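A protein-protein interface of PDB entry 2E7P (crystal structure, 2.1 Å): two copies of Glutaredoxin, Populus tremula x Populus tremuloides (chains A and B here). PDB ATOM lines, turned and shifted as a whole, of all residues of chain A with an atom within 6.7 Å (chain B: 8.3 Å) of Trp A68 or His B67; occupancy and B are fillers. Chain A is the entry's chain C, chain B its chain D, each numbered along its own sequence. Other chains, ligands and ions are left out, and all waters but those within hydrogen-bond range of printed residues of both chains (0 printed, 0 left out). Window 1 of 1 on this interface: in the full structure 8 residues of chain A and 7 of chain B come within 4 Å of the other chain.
Among the printed residues, pairs that only touch across the chains: Ser A63 with Gly B70 (3.2 Å), Ala A66 with Gly B70 (3.4 Å), His A67 with Ala B66 (3.6 Å), His A67 with Trp B68 (3.3 Å), His A67 with Thr B69 (3.5 Å), Thr A69 with His B67 (3.5 Å) and Gly A70 with Ala B66 (3.5 Å).
Of the 19 printed residues of chain B, 6 touch a printed residue of chain A. Hydrophobic or aromatic side chains of chain B within 4 Å of the printed part of chain A: Ala B66 and His B67. Printed residues of chain A that touch a printed residue of chain B: Ser A63, Ala A66, His A67, Trp A68, Thr A69 and Gly A70. Among the printed residues, no Asp or Glu carboxylate lies within 4 Å of a Lys or Arg side-chain nitrogen of the other chain.
The side-chain hydroxyl (OG1) of Thr A69 sits at hydrogen-bond distance from the backbone carbonyl oxygen (O) of Leu A65 (2.6 Å). The side-chain amide oxygen of Gln B83 sits at hydrogen-bond distance from the indole nitrogen of Trp B68 (3.2 Å). OG1 of Thr B69 sits at hydrogen-bond distance from OD1 of Asn B76 (3.2 Å). OG1 of Thr A69 lies within hydrogen-bond range of N of Arg A71, at 3.1 Å. O of Leu B65 is in hydrogen-bond range of OG1 of Thr B69, 2.5 Å away. The backbone NH of Arg B71 sits at hydrogen-bond distance from the side-chain hydroxyl of Thr B69, at 3.1 Å.
Ala A66 touches Gly B70, and with the chains exchanged Gly A70 touches Ala B66. His A67 touches its own counterpart, His B67. His A67 touches Trp B68, and with the chains exchanged Trp A68 touches His B67. His A67 touches Thr B69, and with the chains exchanged Thr A69 touches His B67. Of the 14 pairs that touch across the chains among the printed residues, 14 have their exchanged pair printed and touching as well.
Of chain B, only His B67 comes within 4 Å of Trp A68. His B67 touches just these residues of chain A: Ala A66, His A67, Trp A68, Thr A69 and Gly A70. Printed residues of chain A within 4 Å of Ala B66: Ala A66 (3.4 Å), His A67 (3.6 Å) and Gly A70 (3.5 Å). Of the printed residues of chain B, Gly A70 touches Ser B63 (3.2 Å), Ala B66 (3.5 Å) and His B67 (3.2 Å). Ala A64 touches none of the printed residues of chain B. The nearest residue of chain B that does not touch Trp A68 is Ala B66 (5.8 Å).
NE2 of His B67 lies within hydrogen-bond range of O of Trp A68, 3.3 Å away. The backbone NH (N) of Gly A70 sits at hydrogen-bond distance from a ring nitrogen (NE2) of His B67 (3.2 Å). The backbone NH of Gly B70 sits close to a ring nitrogen (NE2) of His A67. The backbone carbonyl oxygen (O) of Ala B66 lies close to the backbone carbonyl oxygen (O) of Ala A66 (3.5 Å). ND1 of His A67 lies within hydrogen-bond range of O of His B67. N of His B67 is in hydrogen-bond range of O of Ala A66 (3.4 Å). The backbone carbonyl oxygen (O) of Gly A70 lies close to the side-chain hydroxyl (OG) of Ser B63, at 3.2 Å.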
ATOM      1  N   LEU A  10     -24.372 -23.329 -18.836  1.00  0.00           N
ATOM      2  CA  LEU A  10     -25.085 -22.096 -18.614  1.00  0.00           C
ATOM      3  C   LEU A  10     -26.248 -22.335 -17.652  1.00  0.00           C
ATOM      4  O   LEU A  10     -26.487 -21.535 -16.730  1.00  0.00           O
ATOM      5  CB  LEU A  10     -25.597 -21.525 -19.935  1.00  0.00           C
ATOM      6  CG  LEU A  10     -26.428 -20.241 -19.794  1.00  0.00           C
ATOM      7  CD1 LEU A  10     -25.611 -19.105 -19.142  1.00  0.00           C
ATOM      8  CD2 LEU A  10     -26.943 -19.830 -21.153  1.00  0.00           C
ATOM      9  N   ALA A  13     -24.735 -22.834 -14.143  1.00  0.00           N
ATOM     10  CA  ALA A  13     -24.331 -21.520 -13.583  1.00  0.00           C
ATOM     11  C   ALA A  13     -25.518 -20.686 -13.088  1.00  0.00           C
ATOM     12  O   ALA A  13     -25.496 -20.124 -11.987  1.00  0.00           O
ATOM     13  CB  ALA A  13     -23.478 -20.713 -14.601  1.00  0.00           C
ATOM     14  N   LYS A  14     -26.561 -20.587 -13.903  1.00  0.00           N
ATOM     15  CA  LYS A  14     -27.745 -19.825 -13.505  1.00  0.00           C
ATOM     16  C   LYS A  14     -28.406 -20.353 -12.222  1.00  0.00           C
ATOM     17  O   LYS A  14     -28.866 -19.573 -11.391  1.00  0.00           O
ATOM     18  CB  LYS A  14     -28.746 -19.734 -14.651  1.00  0.00           C
ATOM     19  CG  LYS A  14     -28.313 -18.761 -15.753  1.00  0.00           C
ATOM     20  CD  LYS A  14     -29.462 -18.433 -16.698  1.00  0.00           C
ATOM     21  CE  LYS A  14     -28.954 -17.910 -18.040  1.00  0.00           C
ATOM     22  NZ  LYS A  14     -30.033 -17.124 -18.706  1.00  0.00           N
ATOM     23  N   GLU A  15     -28.428 -21.677 -12.077  1.00  0.00           N
ATOM     24  CA  GLU A  15     -28.990 -22.322 -10.909  1.00  0.00           C
ATOM     25  C   GLU A  15     -28.159 -21.983  -9.680  1.00  0.00           C
ATOM     26  O   GLU A  15     -28.696 -21.550  -8.659  1.00  0.00           O
ATOM     27  CB  GLU A  15     -28.989 -23.834 -11.084  1.00  0.00           C
ATOM     28  CG  GLU A  15     -30.061 -24.380 -12.028  1.00  0.00           C
ATOM     29  CD  GLU A  15     -30.040 -25.902 -12.078  1.00  0.00           C
ATOM     30  OE1 GLU A  15     -30.393 -26.522 -11.029  1.00  0.00           O
ATOM     31  OE2 GLU A  15     -29.666 -26.470 -13.149  1.00  0.00           O
ATOM     32  N   ALA A  17     -26.203 -19.520  -9.252  1.00  0.00           N
ATOM     33  CA  ALA A  17     -26.269 -18.068  -8.980  1.00  0.00           C
ATOM     34  C   ALA A  17     -27.481 -17.632  -8.147  1.00  0.00           C
ATOM     35  O   ALA A  17     -27.434 -16.610  -7.424  1.00  0.00           O
ATOM     36  CB  ALA A  17     -26.235 -17.301 -10.282  1.00  0.00           C
ATOM     37  N   SER A  18     -28.564 -18.405  -8.267  1.00  0.00           N
ATOM     38  CA  SER A  18     -29.795 -18.153  -7.508  1.00  0.00           C
ATOM     39  C   SER A  18     -29.960 -19.140  -6.363  1.00  0.00           C
ATOM     40  O   SER A  18     -30.956 -19.084  -5.652  1.00  0.00           O
ATOM     41  CB  SER A  18     -31.006 -18.230  -8.427  1.00  0.00           C
ATOM     42  OG  SER A  18     -31.047 -17.100  -9.270  1.00  0.00           O
ATOM     43  N   PHE A  25     -19.191 -16.596  -6.780  1.00  0.00           N
ATOM     44  CA  PHE A  25     -18.247 -17.380  -7.597  1.00  0.00           C
ATOM     45  C   PHE A  25     -16.810 -16.882  -7.374  1.00  0.00           C
ATOM     46  O   PHE A  25     -16.527 -15.700  -7.456  1.00  0.00           O
ATOM     47  CB  PHE A  25     -18.645 -17.373  -9.088  1.00  0.00           C
ATOM     48  CG  PHE A  25     -20.016 -17.963  -9.352  1.00  0.00           C
ATOM     49  CD1 PHE A  25     -20.176 -19.319  -9.604  1.00  0.00           C
ATOM     50  CD2 PHE A  25     -21.135 -17.148  -9.376  1.00  0.00           C
ATOM     51  CE1 PHE A  25     -21.421 -19.858  -9.891  1.00  0.00           C
ATOM     52  CE2 PHE A  25     -22.395 -17.679  -9.623  1.00  0.00           C
ATOM     53  CZ  PHE A  25     -22.531 -19.045  -9.888  1.00  0.00           C
ATOM     54  N   SER A  63     -16.773 -19.666 -18.181  1.00  0.00           N
ATOM     55  CA  SER A  63     -17.077 -19.097 -19.494  1.00  0.00           C
ATOM     56  C   SER A  63     -18.584 -18.893 -19.697  1.00  0.00           C
ATOM     57  O   SER A  63     -19.000 -17.883 -20.266  1.00  0.00           O
ATOM     58  CB  SER A  63     -16.382 -19.852 -20.653  1.00  0.00           C
ATOM     59  OG  SER A  63     -16.891 -21.148 -20.774  1.00  0.00           O
ATOM     60  N   ALA A  64     -19.411 -19.799 -19.159  1.00  0.00           N
ATOM     61  CA  ALA A  64     -20.864 -19.555 -19.079  1.00  0.00           C
ATOM     62  C   ALA A  64     -21.147 -18.251 -18.338  1.00  0.00           C
ATOM     63  O   ALA A  64     -22.055 -17.499 -18.710  1.00  0.00           O
ATOM     64  CB  ALA A  64     -21.588 -20.720 -18.363  1.00  0.00           C
ATOM     65  N   LEU A  65     -20.419 -17.992 -17.253  1.00  0.00           N
ATOM     66  CA  LEU A  65     -20.655 -16.760 -16.523  1.00  0.00           C
ATOM     67  C   LEU A  65     -20.194 -15.557 -17.352  1.00  0.00           C
ATOM     68  O   LEU A  65     -20.848 -14.513 -17.335  1.00  0.00           O
ATOM     69  CB  LEU A  65     -19.966 -16.764 -15.141  1.00  0.00           C
ATOM     70  CG  LEU A  65     -20.673 -17.568 -14.035  1.00  0.00           C
ATOM     71  CD1 LEU A  65     -19.658 -17.845 -12.902  1.00  0.00           C
ATOM     72  CD2 LEU A  65     -21.873 -16.784 -13.505  1.00  0.00           C
ATOM     73  N   ALA A  66     -19.095 -15.724 -18.077  1.00  0.00           N
ATOM     74  CA  ALA A  66     -18.609 -14.695 -18.987  1.00  0.00           C
ATOM     75  C   ALA A  66     -19.658 -14.348 -20.042  1.00  0.00           C
ATOM     76  O   ALA A  66     -20.058 -13.182 -20.179  1.00  0.00           O
ATOM     77  CB  ALA A  66     -17.307 -15.103 -19.610  1.00  0.00           C
ATOM     78  N   HIS A  67     -20.148 -15.369 -20.743  1.00  0.00           N
ATOM     79  CA  HIS A  67     -21.169 -15.147 -21.781  1.00  0.00           C
ATOM     80  C   HIS A  67     -22.427 -14.500 -21.201  1.00  0.00           C
ATOM     81  O   HIS A  67     -23.043 -13.611 -21.797  1.00  0.00           O
ATOM     82  CB  HIS A  67     -21.550 -16.472 -22.431  1.00  0.00           C
ATOM     83  CG  HIS A  67     -20.587 -16.936 -23.475  1.00  0.00           C
ATOM     84  ND1 HIS A  67     -20.359 -16.236 -24.640  1.00  0.00           N
ATOM     85  CD2 HIS A  67     -19.810 -18.047 -23.542  1.00  0.00           C
ATOM     86  CE1 HIS A  67     -19.478 -16.891 -25.380  1.00  0.00           C
ATOM     87  NE2 HIS A  67     -19.143 -18.003 -24.747  1.00  0.00           N
ATOM     88  N   TRP A  68     -22.816 -14.930 -20.014  1.00  0.00           N
ATOM     89  CA  TRP A  68     -24.103 -14.496 -19.503  1.00  0.00           C
ATOM     90  C   TRP A  68     -24.051 -13.098 -18.881  1.00  0.00           C
ATOM     91  O   TRP A  68     -24.918 -12.238 -19.163  1.00  0.00           O
ATOM     92  CB  TRP A  68     -24.665 -15.584 -18.568  1.00  0.00           C
ATOM     93  CG  TRP A  68     -25.825 -15.203 -17.692  1.00  0.00           C
ATOM     94  CD1 TRP A  68     -26.920 -14.476 -18.049  1.00  0.00           C
ATOM     95  CD2 TRP A  68     -26.036 -15.612 -16.339  1.00  0.00           C
ATOM     96  NE1 TRP A  68     -27.771 -14.346 -16.975  1.00  0.00           N
ATOM     97  CE2 TRP A  68     -27.259 -15.052 -15.920  1.00  0.00           C
ATOM     98  CE3 TRP A  68     -25.296 -16.399 -15.431  1.00  0.00           C
ATOM     99  CZ2 TRP A  68     -27.781 -15.245 -14.615  1.00  0.00           C
ATOM    100  CZ3 TRP A  68     -25.780 -16.561 -14.121  1.00  0.00           C
ATOM    101  CH2 TRP A  68     -27.009 -15.984 -13.726  1.00  0.00           C
ATOM    102  N   THR A  69     -23.028 -12.861 -18.048  1.00  0.00           N
ATOM    103  CA  THR A  69     -22.997 -11.684 -17.190  1.00  0.00           C
ATOM    104  C   THR A  69     -22.073 -10.599 -17.726  1.00  0.00           C
ATOM    105  O   THR A  69     -22.096  -9.433 -17.259  1.00  0.00           O
ATOM    106  CB  THR A  69     -22.537 -12.085 -15.755  1.00  0.00           C
ATOM    107  OG1 THR A  69     -21.153 -12.461 -15.752  1.00  0.00           O
ATOM    108  CG2 THR A  69     -23.365 -13.267 -15.227  1.00  0.00           C
ATOM    109  N   GLY A  70     -21.235 -10.984 -18.679  1.00  0.00           N
ATOM    110  CA  GLY A  70     -20.193 -10.103 -19.160  1.00  0.00           C
ATOM    111  C   GLY A  70     -19.025  -9.946 -18.189  1.00  0.00           C
ATOM    112  O   GLY A  70     -18.175  -9.083 -18.385  1.00  0.00           O
ATOM    113  N   ARG A  71     -19.017 -10.749 -17.136  1.00  0.00           N
ATOM    114  CA  ARG A  71     -17.901 -10.810 -16.159  1.00  0.00           C
ATOM    115  C   ARG A  71     -17.288 -12.204 -16.154  1.00  0.00           C
ATOM    116  O   ARG A  71     -17.913 -13.158 -15.656  1.00  0.00           O
ATOM    117  CB  ARG A  71     -18.382 -10.427 -14.750  1.00  0.00           C
ATOM    118  CG  ARG A  71     -17.281 -10.473 -13.666  1.00  0.00           C
ATOM    119  CD  ARG A  71     -17.808 -10.008 -12.328  1.00  0.00           C
ATOM    120  NE  ARG A  71     -18.223  -8.633 -12.432  1.00  0.00           N
ATOM    121  CZ  ARG A  71     -17.394  -7.590 -12.364  1.00  0.00           C
ATOM    122  NH1 ARG A  71     -16.101  -7.782 -12.094  1.00  0.00           N
ATOM    123  NH2 ARG A  71     -17.870  -6.363 -12.549  1.00  0.00           N
ATOM    124  N   PHE A  78     -23.521 -12.375  -6.692  1.00  0.00           N
ATOM    125  CA  PHE A  78     -24.965 -12.285  -6.859  1.00  0.00           C
ATOM    126  C   PHE A  78     -25.602 -12.107  -5.504  1.00  0.00           C
ATOM    127  O   PHE A  78     -25.246 -12.812  -4.527  1.00  0.00           O
ATOM    128  CB  PHE A  78     -25.497 -13.595  -7.443  1.00  0.00           C
ATOM    129  CG  PHE A  78     -25.191 -13.772  -8.894  1.00  0.00           C
ATOM    130  CD1 PHE A  78     -26.161 -13.480  -9.856  1.00  0.00           C
ATOM    131  CD2 PHE A  78     -23.943 -14.220  -9.303  1.00  0.00           C
ATOM    132  CE1 PHE A  78     -25.879 -13.640 -11.235  1.00  0.00           C
ATOM    133  CE2 PHE A  78     -23.640 -14.385 -10.665  1.00  0.00           C
ATOM    134  CZ  PHE A  78     -24.611 -14.105 -11.634  1.00  0.00           C
ATOM    135  N   GLY A  81     -30.121 -13.321  -6.388  1.00  0.00           N
ATOM    136  CA  GLY A  81     -30.170 -13.779  -7.797  1.00  0.00           C
ATOM    137  C   GLY A  81     -29.867 -12.711  -8.840  1.00  0.00           C
ATOM    138  O   GLY A  81     -29.885 -12.989 -10.028  1.00  0.00           O
ATOM    139  N   GLN A  83     -27.194  -9.897 -10.479  1.00  0.00           N
ATOM    140  CA  GLN A  83     -25.780  -9.631 -10.689  1.00  0.00           C
ATOM    141  C   GLN A  83     -25.354  -8.364  -9.979  1.00  0.00           C
ATOM    142  O   GLN A  83     -25.896  -7.282 -10.240  1.00  0.00           O
ATOM    143  CB  GLN A  83     -25.471  -9.501 -12.178  1.00  0.00           C
ATOM    144  CG  GLN A  83     -25.667 -10.816 -12.908  1.00  0.00           C
ATOM    145  CD  GLN A  83     -25.857 -10.666 -14.393  1.00  0.00           C
ATOM    146  OE1 GLN A  83     -26.725 -11.329 -14.997  1.00  0.00           O
ATOM    147  NE2 GLN A  83     -25.054  -9.798 -15.011  1.00  0.00           N
ATOM    148  N   ASP B   7     -23.136  -3.369 -25.969  1.00  0.00           N
ATOM    149  CA  ASP B   7     -23.774  -3.129 -27.305  1.00  0.00           C
ATOM    150  C   ASP B   7     -22.992  -2.126 -28.189  1.00  0.00           C
ATOM    151  O   ASP B   7     -22.592  -2.453 -29.308  1.00  0.00           O
ATOM    152  CB  ASP B   7     -25.237  -2.696 -27.127  1.00  0.00           C
ATOM    153  CG  ASP B   7     -26.047  -3.690 -26.284  1.00  0.00           C
ATOM    154  OD1 ASP B   7     -25.721  -4.909 -26.322  1.00  0.00           O
ATOM    155  OD2 ASP B   7     -27.009  -3.257 -25.586  1.00  0.00           O
ATOM    156  N   ALA B   9     -20.169  -0.982 -27.004  1.00  0.00           N
ATOM    157  CA  ALA B   9     -18.923  -1.679 -26.733  1.00  0.00           C
ATOM    158  C   ALA B   9     -18.839  -2.994 -27.515  1.00  0.00           C
ATOM    159  O   ALA B   9     -17.778  -3.321 -28.021  1.00  0.00           O
ATOM    160  CB  ALA B   9     -18.736  -1.894 -25.224  1.00  0.00           C
ATOM    161  N   LEU B  10     -19.956  -3.719 -27.651  1.00  0.00           N
ATOM    162  CA  LEU B  10     -19.957  -4.973 -28.435  1.00  0.00           C
ATOM    163  C   LEU B  10     -19.627  -4.722 -29.906  1.00  0.00           C
ATOM    164  O   LEU B  10     -18.846  -5.464 -30.506  1.00  0.00           O
ATOM    165  CB  LEU B  10     -21.267  -5.758 -28.305  1.00  0.00           C
ATOM    166  CG  LEU B  10     -21.119  -7.199 -28.815  1.00  0.00           C
ATOM    167  CD1 LEU B  10     -20.595  -8.123 -27.709  1.00  0.00           C
ATOM    168  CD2 LEU B  10     -22.373  -7.789 -29.441  1.00  0.00           C
ATOM    169  N   LYS B  14     -16.100  -5.870 -31.836  1.00  0.00           N
ATOM    170  CA  LYS B  14     -16.123  -6.710 -33.036  1.00  0.00           C
ATOM    171  C   LYS B  14     -15.370  -6.032 -34.181  1.00  0.00           C
ATOM    172  O   LYS B  14     -14.606  -6.681 -34.885  1.00  0.00           O
ATOM    173  CB  LYS B  14     -17.562  -7.053 -33.428  1.00  0.00           C
ATOM    174  CG  LYS B  14     -18.183  -8.164 -32.564  1.00  0.00           C
ATOM    175  CD  LYS B  14     -19.706  -8.206 -32.759  1.00  0.00           C
ATOM    176  CE  LYS B  14     -20.360  -9.432 -32.095  1.00  0.00           C
ATOM    177  NZ  LYS B  14     -20.743 -10.462 -33.122  1.00  0.00           N
ATOM    178  N   GLN B  60     -16.032  -1.615 -20.280  1.00  0.00           N
ATOM    179  CA  GLN B  60     -17.172  -1.979 -21.135  1.00  0.00           C
ATOM    180  C   GLN B  60     -16.746  -2.885 -22.284  1.00  0.00           C
ATOM    181  O   GLN B  60     -17.457  -3.841 -22.638  1.00  0.00           O
ATOM    182  CB  GLN B  60     -17.872  -0.711 -21.692  1.00  0.00           C
ATOM    183  CG  GLN B  60     -18.470   0.198 -20.575  1.00  0.00           C
ATOM    184  CD  GLN B  60     -17.521   1.320 -20.108  1.00  0.00           C
ATOM    185  OE1 GLN B  60     -16.414   1.067 -19.551  1.00  0.00           O
ATOM    186  NE2 GLN B  60     -17.952   2.585 -20.339  1.00  0.00           N
ATOM    187  N   LEU B  61     -15.595  -2.577 -22.874  1.00  0.00           N
ATOM    188  CA  LEU B  61     -15.041  -3.369 -23.952  1.00  0.00           C
ATOM    189  C   LEU B  61     -14.682  -4.786 -23.499  1.00  0.00           C
ATOM    190  O   LEU B  61     -14.937  -5.741 -24.232  1.00  0.00           O
ATOM    191  CB  LEU B  61     -13.814  -2.687 -24.570  1.00  0.00           C
ATOM    192  CG  LEU B  61     -14.008  -1.547 -25.582  1.00  0.00           C
ATOM    193  CD1 LEU B  61     -12.686  -0.930 -25.990  1.00  0.00           C
ATOM    194  CD2 LEU B  61     -14.798  -2.009 -26.813  1.00  0.00           C
ATOM    195  N   GLN B  62     -14.086  -4.903 -22.309  1.00  0.00           N
ATOM    196  CA  GLN B  62     -13.740  -6.194 -21.706  1.00  0.00           C
ATOM    197  C   GLN B  62     -14.988  -7.038 -21.437  1.00  0.00           C
ATOM    198  O   GLN B  62     -15.017  -8.260 -21.653  1.00  0.00           O
ATOM    199  CB  GLN B  62     -12.970  -5.978 -20.388  1.00  0.00           C
ATOM    200  CG  GLN B  62     -12.359  -7.270 -19.786  1.00  0.00           C
ATOM    201  CD  GLN B  62     -11.436  -7.031 -18.604  1.00  0.00           C
ATOM    202  OE1 GLN B  62     -11.168  -5.882 -18.214  1.00  0.00           O
ATOM    203  NE2 GLN B  62     -10.953  -8.133 -18.006  1.00  0.00           N
ATOM    204  N   SER B  63     -16.017  -6.361 -20.976  1.00  0.00           N
ATOM    205  CA  SER B  63     -17.291  -6.981 -20.696  1.00  0.00           C
ATOM    206  C   SER B  63     -17.989  -7.444 -22.002  1.00  0.00           C
ATOM    207  O   SER B  63     -18.524  -8.549 -22.069  1.00  0.00           O
ATOM    208  CB  SER B  63     -18.111  -5.993 -19.841  1.00  0.00           C
ATOM    209  OG  SER B  63     -19.439  -6.398 -19.703  1.00  0.00           O
ATOM    210  N   ALA B  64     -17.914  -6.632 -23.052  1.00  0.00           N
ATOM    211  CA  ALA B  64     -18.347  -7.046 -24.393  1.00  0.00           C
ATOM    212  C   ALA B  64     -17.620  -8.315 -24.885  1.00  0.00           C
ATOM    213  O   ALA B  64     -18.250  -9.272 -25.352  1.00  0.00           O
ATOM    214  CB  ALA B  64     -18.179  -5.888 -25.381  1.00  0.00           C
ATOM    215  N   LEU B  65     -16.299  -8.345 -24.740  1.00  0.00           N
ATOM    216  CA  LEU B  65     -15.524  -9.540 -25.073  1.00  0.00           C
ATOM    217  C   LEU B  65     -15.877 -10.815 -24.282  1.00  0.00           C
ATOM    218  O   LEU B  65     -15.840 -11.925 -24.838  1.00  0.00           O
ATOM    219  CB  LEU B  65     -14.022  -9.253 -24.951  1.00  0.00           C
ATOM    220  CG  LEU B  65     -13.478  -8.287 -26.017  1.00  0.00           C
ATOM    221  CD1 LEU B  65     -12.185  -7.603 -25.535  1.00  0.00           C
ATOM    222  CD2 LEU B  65     -13.276  -9.030 -27.371  1.00  0.00           C
ATOM    223  N   ALA B  66     -16.151 -10.669 -22.986  1.00  0.00           N
ATOM    224  CA  ALA B  66     -16.626 -11.782 -22.158  1.00  0.00           C
ATOM    225  C   ALA B  66     -17.961 -12.278 -22.719  1.00  0.00           C
ATOM    226  O   ALA B  66     -18.086 -13.473 -23.036  1.00  0.00           O
ATOM    227  CB  ALA B  66     -16.795 -11.328 -20.716  1.00  0.00           C
ATOM    228  N   HIS B  67     -18.943 -11.374 -22.855  1.00  0.00           N
ATOM    229  CA  HIS B  67     -20.237 -11.715 -23.453  1.00  0.00           C
ATOM    230  C   HIS B  67     -20.082 -12.509 -24.779  1.00  0.00           C
ATOM    231  O   HIS B  67     -20.661 -13.587 -24.960  1.00  0.00           O
ATOM    232  CB  HIS B  67     -21.088 -10.449 -23.703  1.00  0.00           C
ATOM    233  CG  HIS B  67     -21.939 -10.030 -22.541  1.00  0.00           C
ATOM    234  ND1 HIS B  67     -21.923  -8.745 -22.032  1.00  0.00           N
ATOM    235  CD2 HIS B  67     -22.842 -10.713 -21.796  1.00  0.00           C
ATOM    236  CE1 HIS B  67     -22.767  -8.658 -21.017  1.00  0.00           C
ATOM    237  NE2 HIS B  67     -23.337  -9.837 -20.853  1.00  0.00           N
ATOM    238  N   TRP B  68     -19.250 -11.988 -25.674  1.00  0.00           N
ATOM    239  CA  TRP B  68     -19.119 -12.523 -27.029  1.00  0.00           C
ATOM    240  C   TRP B  68     -18.238 -13.776 -27.094  1.00  0.00           C
ATOM    241  O   TRP B  68     -18.612 -14.803 -27.720  1.00  0.00           O
ATOM    242  CB  TRP B  68     -18.615 -11.387 -27.944  1.00  0.00           C
ATOM    243  CG  TRP B  68     -18.129 -11.745 -29.325  1.00  0.00           C
ATOM    244  CD1 TRP B  68     -18.595 -12.758 -30.152  1.00  0.00           C
ATOM    245  CD2 TRP B  68     -17.120 -11.059 -30.070  1.00  0.00           C
ATOM    246  NE1 TRP B  68     -17.895 -12.753 -31.344  1.00  0.00           N
ATOM    247  CE2 TRP B  68     -16.992 -11.724 -31.323  1.00  0.00           C
ATOM    248  CE3 TRP B  68     -16.310  -9.949 -29.807  1.00  0.00           C
ATOM    249  CZ2 TRP B  68     -16.080 -11.310 -32.300  1.00  0.00           C
ATOM    250  CZ3 TRP B  68     -15.403  -9.543 -30.774  1.00  0.00           C
ATOM    251  CH2 TRP B  68     -15.289 -10.223 -32.001  1.00  0.00           C
ATOM    252  N   THR B  69     -17.072 -13.729 -26.435  1.00  0.00           N
ATOM    253  CA  THR B  69     -16.092 -14.798 -26.592  1.00  0.00           C
ATOM    254  C   THR B  69     -16.135 -15.847 -25.482  1.00  0.00           C
ATOM    255  O   THR B  69     -15.548 -16.901 -25.650  1.00  0.00           O
ATOM    256  CB  THR B  69     -14.640 -14.246 -26.667  1.00  0.00           C
ATOM    257  OG1 THR B  69     -14.245 -13.717 -25.391  1.00  0.00           O
ATOM    258  CG2 THR B  69     -14.468 -13.163 -27.765  1.00  0.00           C
ATOM    259  N   GLY B  70     -16.760 -15.547 -24.336  1.00  0.00           N
ATOM    260  CA  GLY B  70     -16.622 -16.410 -23.131  1.00  0.00           C
ATOM    261  C   GLY B  70     -15.304 -16.305 -22.331  1.00  0.00           C
ATOM    262  O   GLY B  70     -15.113 -17.005 -21.337  1.00  0.00           O
ATOM    263  N   ARG B  71     -14.402 -15.429 -22.754  1.00  0.00           N
ATOM    264  CA  ARG B  71     -13.140 -15.178 -22.056  1.00  0.00           C
ATOM    265  C   ARG B  71     -13.205 -13.803 -21.412  1.00  0.00           C
ATOM    266  O   ARG B  71     -13.450 -12.818 -22.103  1.00  0.00           O
ATOM    267  CB  ARG B  71     -11.976 -15.226 -23.055  1.00  0.00           C
ATOM    268  CG  ARG B  71     -10.593 -14.735 -22.552  1.00  0.00           C
ATOM    269  CD  ARG B  71      -9.565 -15.011 -23.635  1.00  0.00           C
ATOM    270  NE  ARG B  71      -9.493 -16.448 -23.915  1.00  0.00           N
ATOM    271  CZ  ARG B  71      -8.821 -17.365 -23.209  1.00  0.00           C
ATOM    272  NH1 ARG B  71      -8.087 -17.058 -22.138  1.00  0.00           N
ATOM    273  NH2 ARG B  71      -8.898 -18.631 -23.586  1.00  0.00           N
ATOM    274  N   GLY B  72     -12.952 -13.739 -20.105  1.00  0.00           N
ATOM    275  CA  GLY B  72     -13.072 -12.487 -19.373  1.00  0.00           C
ATOM    276  C   GLY B  72     -11.750 -11.838 -18.986  1.00  0.00           C
ATOM    277  O   GLY B  72     -11.732 -10.871 -18.211  1.00  0.00           O
ATOM    278  N   ASN B  76      -6.720 -11.378 -25.175  1.00  0.00           N
ATOM    279  CA  ASN B  76      -7.774 -11.979 -25.983  1.00  0.00           C
ATOM    280  C   ASN B  76      -7.319 -11.792 -27.434  1.00  0.00           C
ATOM    281  O   ASN B  76      -7.283 -10.659 -27.970  1.00  0.00           O
ATOM    282  CB  ASN B  76      -9.131 -11.317 -25.678  1.00  0.00           C
ATOM    283  CG  ASN B  76     -10.342 -12.236 -25.991  1.00  0.00           C
ATOM    284  OD1 ASN B  76     -11.404 -12.155 -25.342  1.00  0.00           O
ATOM    285  ND2 ASN B  76     -10.194 -13.081 -26.993  1.00  0.00           N
ATOM    286  N   GLN B  83     -11.562 -15.668 -33.248  1.00  0.00           N
ATOM    287  CA  GLN B  83     -11.143 -15.910 -31.853  1.00  0.00           C
ATOM    288  C   GLN B  83     -10.121 -17.045 -31.749  1.00  0.00           C
ATOM    289  O   GLN B  83     -10.392 -18.165 -32.192  1.00  0.00           O
ATOM    290  CB  GLN B  83     -12.355 -16.259 -30.976  1.00  0.00           C
ATOM    291  CG  GLN B  83     -13.381 -15.127 -30.821  1.00  0.00           C
ATOM    292  CD  GLN B  83     -14.797 -15.598 -30.407  1.00  0.00           C
ATOM    293  OE1 GLN B  83     -15.809 -15.076 -30.906  1.00  0.00           O
ATOM    294  NE2 GLN B  83     -14.871 -16.569 -29.489  1.00  0.00           N
